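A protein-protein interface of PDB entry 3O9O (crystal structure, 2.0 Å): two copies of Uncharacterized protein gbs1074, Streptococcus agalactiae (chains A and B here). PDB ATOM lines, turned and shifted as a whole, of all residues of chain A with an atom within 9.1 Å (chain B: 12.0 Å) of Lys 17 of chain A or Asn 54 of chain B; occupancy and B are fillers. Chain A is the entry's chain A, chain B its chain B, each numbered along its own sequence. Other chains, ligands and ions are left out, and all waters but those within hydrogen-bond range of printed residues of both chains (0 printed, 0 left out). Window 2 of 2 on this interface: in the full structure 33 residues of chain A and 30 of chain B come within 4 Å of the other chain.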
ATOM      1  N   ILE A  16      29.687   3.357 -15.625  1.00  0.00           N
ATOM      2  CA  ILE A  16      28.352   3.583 -15.089  1.00  0.00           C
ATOM      3  C   ILE A  16      28.119   5.071 -14.839  1.00  0.00           C
ATOM      4  O   ILE A  16      28.812   5.689 -14.034  1.00  0.00           O
ATOM      5  CB  ILE A  16      28.135   2.799 -13.774  1.00  0.00           C
ATOM      6  CG1 ILE A  16      28.276   1.297 -14.024  1.00  0.00           C
ATOM      7  CG2 ILE A  16      26.768   3.104 -13.182  1.00  0.00           C
ATOM      8  CD1 ILE A  16      27.595   0.426 -12.978  1.00  0.00           C
ATOM      9  N   LYS A  17      27.140   5.639 -15.540  1.00  0.00           N
ATOM     10  CA  LYS A  17      26.801   7.054 -15.409  1.00  0.00           C
ATOM     11  C   LYS A  17      25.886   7.325 -14.214  1.00  0.00           C
ATOM     12  O   LYS A  17      25.442   8.456 -14.011  1.00  0.00           O
ATOM     13  CB  LYS A  17      26.094   7.552 -16.675  1.00  0.00           C
ATOM     14  CG  LYS A  17      26.982   7.769 -17.892  1.00  0.00           C
ATOM     15  CD  LYS A  17      26.143   8.266 -19.069  1.00  0.00           C
ATOM     16  CE  LYS A  17      26.994   8.803 -20.208  1.00  0.00           C
ATOM     17  NZ  LYS A  17      26.149   9.299 -21.333  1.00  0.00           N
ATOM     18  N   LEU A  18      25.590   6.290 -13.438  1.00  0.00           N
ATOM     19  CA  LEU A  18      24.668   6.420 -12.315  1.00  0.00           C
ATOM     20  C   LEU A  18      25.419   6.504 -10.996  1.00  0.00           C
ATOM     21  O   LEU A  18      26.313   5.714 -10.736  1.00  0.00           O
ATOM     22  CB  LEU A  18      23.709   5.227 -12.276  1.00  0.00           C
ATOM     23  CG  LEU A  18      22.763   5.106 -13.472  1.00  0.00           C
ATOM     24  CD1 LEU A  18      22.071   3.752 -13.470  1.00  0.00           C
ATOM     25  CD2 LEU A  18      21.747   6.239 -13.476  1.00  0.00           C
ATOM     26  N   THR A  19      25.044   7.464 -10.162  1.00  0.00           N
ATOM     27  CA  THR A  19      25.634   7.593  -8.836  1.00  0.00           C
ATOM     28  C   THR A  19      25.089   6.512  -7.882  1.00  0.00           C
ATOM     29  O   THR A  19      24.084   5.851  -8.183  1.00  0.00           O
ATOM     30  CB  THR A  19      25.299   8.962  -8.241  1.00  0.00           C
ATOM     31  OG1 THR A  19      23.884   9.048  -8.046  1.00  0.00           O
ATOM     32  CG2 THR A  19      25.737  10.084  -9.172  1.00  0.00           C
ATOM     33  N   PRO A  20      25.743   6.338  -6.724  1.00  0.00           N
ATOM     34  CA  PRO A  20      25.208   5.402  -5.735  1.00  0.00           C
ATOM     35  C   PRO A  20      23.779   5.751  -5.336  1.00  0.00           C
ATOM     36  O   PRO A  20      22.957   4.858  -5.167  1.00  0.00           O
ATOM     37  CB  PRO A  20      26.156   5.565  -4.558  1.00  0.00           C
ATOM     38  CG  PRO A  20      27.486   5.907  -5.217  1.00  0.00           C
ATOM     39  CD  PRO A  20      27.095   6.815  -6.366  1.00  0.00           C
ATOM     40  N   GLU A  22      21.433   7.270  -7.144  1.00  0.00           N
ATOM     41  CA  GLU A  22      20.526   6.907  -8.239  1.00  0.00           C
ATOM     42  C   GLU A  22      20.328   5.400  -8.303  1.00  0.00           C
ATOM     43  O   GLU A  22      19.221   4.916  -8.550  1.00  0.00           O
ATOM     44  CB  GLU A  22      21.070   7.409  -9.579  1.00  0.00           C
ATOM     45  CG  GLU A  22      20.859   8.905  -9.800  1.00  0.00           C
ATOM     46  CD  GLU A  22      21.677   9.471 -10.952  1.00  0.00           C
ATOM     47  OE1 GLU A  22      22.650   8.821 -11.394  1.00  0.00           O
ATOM     48  OE2 GLU A  22      21.349  10.586 -11.402  1.00  0.00           O
ATOM     49  N   LEU A  23      21.406   4.656  -8.093  1.00  0.00           N
ATOM     50  CA  LEU A  23      21.321   3.204  -8.067  1.00  0.00           C
ATOM     51  C   LEU A  23      20.407   2.736  -6.927  1.00  0.00           C
ATOM     52  O   LEU A  23      19.643   1.787  -7.088  1.00  0.00           O
ATOM     53  CB  LEU A  23      22.711   2.586  -7.922  1.00  0.00           C
ATOM     54  CG  LEU A  23      23.622   2.656  -9.162  1.00  0.00           C
ATOM     55  CD1 LEU A  23      25.088   2.530  -8.761  1.00  0.00           C
ATOM     56  CD2 LEU A  23      23.262   1.587 -10.194  1.00  0.00           C
ATOM     57  N   VAL A  91      26.432  -2.888  -6.156  1.00  0.00           N
ATOM     58  CA  VAL A  91      27.143  -2.029  -7.091  1.00  0.00           C
ATOM     59  C   VAL A  91      27.239  -0.620  -6.515  1.00  0.00           C
ATOM     60  O   VAL A  91      28.290   0.032  -6.610  1.00  0.00           O
ATOM     61  CB  VAL A  91      26.455  -1.984  -8.482  1.00  0.00           C
ATOM     62  CG1 VAL A  91      27.145  -0.963  -9.404  1.00  0.00           C
ATOM     63  CG2 VAL A  91      26.490  -3.346  -9.124  1.00  0.00           C
ATOM     64  N   ILE A  95      30.647   1.591  -5.858  1.00  0.00           N
ATOM     65  CA  ILE A  95      30.874   2.888  -6.479  1.00  0.00           C
ATOM     66  C   ILE A  95      31.020   4.005  -5.453  1.00  0.00           C
ATOM     67  O   ILE A  95      31.789   4.943  -5.651  1.00  0.00           O
ATOM     68  CB  ILE A  95      29.772   3.227  -7.505  1.00  0.00           C
ATOM     69  CG1 ILE A  95      29.843   2.233  -8.670  1.00  0.00           C
ATOM     70  CG2 ILE A  95      29.944   4.655  -8.013  1.00  0.00           C
ATOM     71  CD1 ILE A  95      28.740   2.401  -9.699  1.00  0.00           C
ATOM     72  N   THR B  45       9.861  -1.616 -16.342  1.00  0.00           N
ATOM     73  CA  THR B  45      10.239  -1.705 -17.741  1.00  0.00           C
ATOM     74  C   THR B  45      11.058  -0.467 -18.090  1.00  0.00           C
ATOM     75  O   THR B  45      12.076  -0.541 -18.783  1.00  0.00           O
ATOM     76  CB  THR B  45       8.990  -1.776 -18.636  1.00  0.00           C
ATOM     77  OG1 THR B  45       8.411  -3.083 -18.527  1.00  0.00           O
ATOM     78  CG2 THR B  45       9.347  -1.497 -20.088  1.00  0.00           C
ATOM     79  N   GLN B  46      10.598   0.669 -17.583  1.00  0.00           N
ATOM     80  CA  GLN B  46      11.283   1.941 -17.745  1.00  0.00           C
ATOM     81  C   GLN B  46      12.619   1.983 -16.992  1.00  0.00           C
ATOM     82  O   GLN B  46      13.632   2.437 -17.548  1.00  0.00           O
ATOM     83  CB  GLN B  46      10.367   3.064 -17.265  1.00  0.00           C
ATOM     84  CG  GLN B  46      11.073   4.377 -16.990  1.00  0.00           C
ATOM     85  CD  GLN B  46      10.158   5.399 -16.345  1.00  0.00           C
ATOM     86  OE1 GLN B  46       8.976   5.490 -16.682  1.00  0.00           O
ATOM     87  NE2 GLN B  46      10.699   6.171 -15.408  1.00  0.00           N
ATOM     88  N   GLU B  47      12.631   1.532 -15.735  1.00  0.00           N
ATOM     89  CA  GLU B  47      13.875   1.482 -14.967  1.00  0.00           C
ATOM     90  C   GLU B  47      14.891   0.670 -15.729  1.00  0.00           C
ATOM     91  O   GLU B  47      16.059   1.012 -15.774  1.00  0.00           O
ATOM     92  CB  GLU B  47      13.697   0.831 -13.589  1.00  0.00           C
ATOM     93  CG  GLU B  47      13.173   1.746 -12.490  1.00  0.00           C
ATOM     94  CD  GLU B  47      13.900   3.068 -12.413  1.00  0.00           C
ATOM     95  OE1 GLU B  47      15.072   3.086 -11.992  1.00  0.00           O
ATOM     96  OE2 GLU B  47      13.293   4.098 -12.762  1.00  0.00           O
ATOM     97  N   GLN B  48      14.431  -0.427 -16.310  1.00  0.00           N
ATOM     98  CA  GLN B  48      15.309  -1.338 -17.012  1.00  0.00           C
ATOM     99  C   GLN B  48      16.033  -0.586 -18.139  1.00  0.00           C
ATOM    100  O   GLN B  48      17.219  -0.816 -18.396  1.00  0.00           O
ATOM    101  CB  GLN B  48      14.485  -2.510 -17.550  1.00  0.00           C
ATOM    102  CG  GLN B  48      15.265  -3.782 -17.789  1.00  0.00           C
ATOM    103  CD  GLN B  48      15.561  -4.565 -16.519  1.00  0.00           C
ATOM    104  OE1 GLN B  48      15.564  -4.028 -15.405  1.00  0.00           O
ATOM    105  NE2 GLN B  48      15.832  -5.851 -16.689  1.00  0.00           N
ATOM    106  N   ALA B  49      15.323   0.340 -18.782  1.00  0.00           N
ATOM    107  CA  ALA B  49      15.891   1.126 -19.881  1.00  0.00           C
ATOM    108  C   ALA B  49      16.797   2.263 -19.406  1.00  0.00           C
ATOM    109  O   ALA B  49      17.754   2.614 -20.087  1.00  0.00           O
ATOM    110  CB  ALA B  49      14.787   1.682 -20.750  1.00  0.00           C
ATOM    111  N   VAL B  50      16.476   2.855 -18.259  1.00  0.00           N
ATOM    112  CA  VAL B  50      17.337   3.860 -17.643  1.00  0.00           C
ATOM    113  C   VAL B  50      18.680   3.234 -17.310  1.00  0.00           C
ATOM    114  O   VAL B  50      19.740   3.821 -17.554  1.00  0.00           O
ATOM    115  CB  VAL B  50      16.727   4.409 -16.337  1.00  0.00           C
ATOM    116  CG1 VAL B  50      17.804   5.048 -15.475  1.00  0.00           C
ATOM    117  CG2 VAL B  50      15.615   5.401 -16.632  1.00  0.00           C
ATOM    118  N   ILE B  51      18.629   2.037 -16.736  1.00  0.00           N
ATOM    119  CA  ILE B  51      19.837   1.312 -16.380  1.00  0.00           C
ATOM    120  C   ILE B  51      20.630   0.987 -17.645  1.00  0.00           C
ATOM    121  O   ILE B  51      21.802   1.352 -17.765  1.00  0.00           O
ATOM    122  CB  ILE B  51      19.505   0.025 -15.603  1.00  0.00           C
ATOM    123  CG1 ILE B  51      18.854   0.372 -14.262  1.00  0.00           C
ATOM    124  CG2 ILE B  51      20.761  -0.799 -15.362  1.00  0.00           C
ATOM    125  CD1 ILE B  51      18.381  -0.837 -13.479  1.00  0.00           C
ATOM    126  N   ASP B  52      19.977   0.323 -18.594  1.00  0.00           N
ATOM    127  CA  ASP B  52      20.598  -0.063 -19.860  1.00  0.00           C
ATOM    128  C   ASP B  52      21.329   1.098 -20.531  1.00  0.00           C
ATOM    129  O   ASP B  52      22.477   0.959 -20.959  1.00  0.00           O
ATOM    130  CB  ASP B  52      19.537  -0.609 -20.818  1.00  0.00           C
ATOM    131  CG  ASP B  52      20.102  -0.959 -22.178  1.00  0.00           C
ATOM    132  OD1 ASP B  52      21.204  -1.541 -22.231  1.00  0.00           O
ATOM    133  OD2 ASP B  52      19.441  -0.661 -23.195  1.00  0.00           O
ATOM    134  N   GLU B  53      20.653   2.237 -20.630  1.00  0.00           N
ATOM    135  CA  GLU B  53      21.215   3.418 -21.271  1.00  0.00           C
ATOM    136  C   GLU B  53      22.408   3.974 -20.498  1.00  0.00           C
ATOM    137  O   GLU B  53      23.402   4.392 -21.094  1.00  0.00           O
ATOM    138  CB  GLU B  53      20.151   4.504 -21.394  1.00  0.00           C
ATOM    139  CG  GLU B  53      19.158   4.266 -22.512  1.00  0.00           C
ATOM    140  CD  GLU B  53      17.883   5.060 -22.324  1.00  0.00           C
ATOM    141  OE1 GLU B  53      16.847   4.665 -22.900  1.00  0.00           O
ATOM    142  OE2 GLU B  53      17.917   6.071 -21.592  1.00  0.00           O
ATOM    143  N   ASN B  54      22.300   3.970 -19.170  1.00  0.00           N
ATOM    144  CA  ASN B  54      23.286   4.609 -18.305  1.00  0.00           C
ATOM    145  C   ASN B  54      24.309   3.637 -17.728  1.00  0.00           C
ATOM    146  O   ASN B  54      24.898   3.901 -16.681  1.00  0.00           O
ATOM    147  CB  ASN B  54      22.580   5.331 -17.153  1.00  0.00           C
ATOM    148  CG  ASN B  54      21.889   6.604 -17.594  1.00  0.00           C
ATOM    149  OD1 ASN B  54      22.348   7.706 -17.292  1.00  0.00           O
ATOM    150  ND2 ASN B  54      20.778   6.464 -18.306  1.00  0.00           N
ATOM    151  N   TRP B  55      24.526   2.514 -18.406  1.00  0.00           N
ATOM    152  CA  TRP B  55      25.460   1.504 -17.915  1.00  0.00           C
ATOM    153  C   TRP B  55      25.863   0.538 -19.028  1.00  0.00           C
ATOM    154  O   TRP B  55      25.118  -0.382 -19.362  1.00  0.00           O
ATOM    155  CB  TRP B  55      24.827   0.737 -16.752  1.00  0.00           C
ATOM    156  CG  TRP B  55      25.719  -0.286 -16.112  1.00  0.00           C
ATOM    157  CD1 TRP B  55      26.991  -0.614 -16.476  1.00  0.00           C
ATOM    158  CD2 TRP B  55      25.396  -1.112 -14.988  1.00  0.00           C
ATOM    159  NE1 TRP B  55      27.483  -1.595 -15.647  1.00  0.00           N
ATOM    160  CE2 TRP B  55      26.523  -1.919 -14.724  1.00  0.00           C
ATOM    161  CE3 TRP B  55      24.266  -1.251 -14.176  1.00  0.00           C
ATOM    162  CZ2 TRP B  55      26.550  -2.848 -13.684  1.00  0.00           C
ATOM    163  CZ3 TRP B  55      24.294  -2.176 -13.146  1.00  0.00           C
ATOM    164  CH2 TRP B  55      25.427  -2.962 -12.911  1.00  0.00           C
ATOM    165  N   ASP B  56      27.040   0.755 -19.605  1.00  0.00           N
ATOM    166  CA  ASP B  56      27.543  -0.125 -20.653  1.00  0.00           C
ATOM    167  C   ASP B  56      28.258  -1.329 -20.052  1.00  0.00           C
ATOM    168  O   ASP B  56      28.740  -1.276 -18.922  1.00  0.00           O
ATOM    169  CB  ASP B  56      28.479   0.638 -21.591  1.00  0.00           C
ATOM    170  CG  ASP B  56      27.730   1.381 -22.677  1.00  0.00           C
ATOM    171  OD1 ASP B  56      27.843   2.623 -22.735  1.00  0.00           O
ATOM    172  OD2 ASP B  56      27.024   0.722 -23.470  1.00  0.00           O
ATOM    173  N   GLY B  57      28.323  -2.413 -20.815  1.00  0.00           N
ATOM    174  CA  GLY B  57      28.919  -3.647 -20.336  1.00  0.00           C
ATOM    175  C   GLY B  57      27.917  -4.782 -20.383  1.00  0.00           C
ATOM    176  O   GLY B  57      26.767  -4.584 -20.767  1.00  0.00           O
ATOM    177  N   SER B  58      28.355  -5.973 -19.987  1.00  0.00           N
ATOM    178  CA  SER B  58      27.510  -7.161 -20.044  1.00  0.00           C
ATOM    179  C   SER B  58      27.032  -7.561 -18.656  1.00  0.00           C
ATOM    180  O   SER B  58      26.431  -8.618 -18.477  1.00  0.00           O
ATOM    181  CB  SER B  58      28.297  -8.329 -20.635  1.00  0.00           C
ATOM    182  OG  SER B  58      29.163  -8.886 -19.659  1.00  0.00           O
ATOM    183  N   THR B  59      27.304  -6.709 -17.677  1.00  0.00           N
ATOM    184  CA  THR B  59      27.160  -7.089 -16.275  1.00  0.00           C
ATOM    185  C   THR B  59      25.711  -7.361 -15.828  1.00  0.00           C
ATOM    186  O   THR B  59      25.496  -8.070 -14.845  1.00  0.00           O
ATOM    187  CB  THR B  59      27.842  -6.054 -15.342  1.00  0.00           C
ATOM    188  OG1 THR B  59      27.345  -6.200 -14.006  1.00  0.00           O
ATOM    189  CG2 THR B  59      27.600  -4.631 -15.823  1.00  0.00           C
ATOM    190  N   PHE B  60      24.727  -6.822 -16.545  1.00  0.00           N
ATOM    191  CA  PHE B  60      23.317  -7.073 -16.211  1.00  0.00           C
ATOM    192  C   PHE B  60      22.573  -7.734 -17.365  1.00  0.00           C
ATOM    193  O   PHE B  60      21.345  -7.742 -17.398  1.00  0.00           O
ATOM    194  CB  PHE B  60      22.609  -5.768 -15.838  1.00  0.00           C
ATOM    195  CG  PHE B  60      22.546  -5.507 -14.359  1.00  0.00           C
ATOM    196  CD1 PHE B  60      23.601  -5.849 -13.531  1.00  0.00           C
ATOM    197  CD2 PHE B  60      21.430  -4.902 -13.800  1.00  0.00           C
ATOM    198  CE1 PHE B  60      23.544  -5.604 -12.171  1.00  0.00           C
ATOM    199  CE2 PHE B  60      21.368  -4.653 -12.442  1.00  0.00           C
ATOM    200  CZ  PHE B  60      22.427  -5.004 -11.627  1.00  0.00           C
ATOM    201  N   ASP B  61      23.321  -8.287 -18.312  1.00  0.00           N
ATOM    202  CA  ASP B  61      22.726  -8.893 -19.495  1.00  0.00           C
ATOM    203  C   ASP B  61      21.818 -10.072 -19.159  1.00  0.00           C
ATOM    204  O   ASP B  61      20.850 -10.323 -19.867  1.00  0.00           O
ATOM    205  CB  ASP B  61      23.817  -9.349 -20.472  1.00  0.00           C
ATOM    206  CG  ASP B  61      24.437  -8.194 -21.239  1.00  0.00           C
ATOM    207  OD1 ASP B  61      23.902  -7.068 -21.173  1.00  0.00           O
ATOM    208  OD2 ASP B  61      25.460  -8.418 -21.918  1.00  0.00           O
ATOM    209  N   GLU B  64      18.545  -8.577 -17.814  1.00  0.00           N
ATOM    210  CA  GLU B  64      17.713  -7.986 -18.851  1.00  0.00           C
ATOM    211  C   GLU B  64      16.999  -9.065 -19.662  1.00  0.00           C
ATOM    212  O   GLU B  64      15.842  -8.895 -20.051  1.00  0.00           O
ATOM    213  CB  GLU B  64      18.534  -7.077 -19.764  1.00  0.00           C
ATOM    214  CG  GLU B  64      17.824  -6.724 -21.060  1.00  0.00           C
ATOM    215  CD  GLU B  64      18.416  -5.509 -21.743  1.00  0.00           C
ATOM    216  OE1 GLU B  64      19.372  -5.673 -22.533  1.00  0.00           O
ATOM    217  OE2 GLU B  64      17.924  -4.389 -21.489  1.00  0.00           O
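Of the 9 printed residues of chain A, 4 touch a printed residue of chain B.
Hydrophobic or aromatic side chains of chain A that line the printed part of chain B: Ile 16, Leu 18 and Val 91.
Among the printed residues, 5 pairs touch across the chains.
Among the printed residues, no Asp or Glu carboxylate lies within 4 Å of a Lys or Arg side-chain nitrogen of the other chain.
Of the printed residues of chain B, Lys 17 of chain A touches Asn 54.
Asn 54 of chain B touches just these residues of chain A: Ile 16 (3.8 Å), Lys 17 (3.1 Å) and Leu 18 (3.7 Å).
Of chain B, only Asn 54 (3.8 Å) and Trp 55 (3.1 Å) come within 4 Å of Ile 16 of chain A.
Leu 18 of chain A touches one residue of chain B.
No residue of chain B comes within 4 Å of Thr 19 of chain A.
Printed residues of chain A within 4 Å of Trp 55 of chain B: Ile 16 and Val 91.
Printed residues of chain B within 4 Å of Val 91 of chain A: Trp 55.
Gly 57 of chain B touches none of the printed residues of chain A.
Among the printed residues, merely in contact across the chains: Ile 16 of chain A with Trp 55 of chain B (3.1 Å), Leu 18 of chain A with Asn 54 of chain B (3.7 Å), Ile 16 of chain A with Asn 54 of chain B (3.8 Å) and Val 91 of chain A with Trp 55 of chain B (3.95 Å).
No position is printed for both chains.
Of the 5 pairs that touch across the chains among the printed residues, none has its exchanged pair printed and touching as well.
The backbone carbonyl oxygen (O) of Val 50 of chain B lies within hydrogen-bond range of the side-chain amide nitrogen (ND2) of Asn 54 of chain B.
N of Lys 17 of chain A lies within hydrogen-bond range of O of Asn 54 of chain B (3.1 Å).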
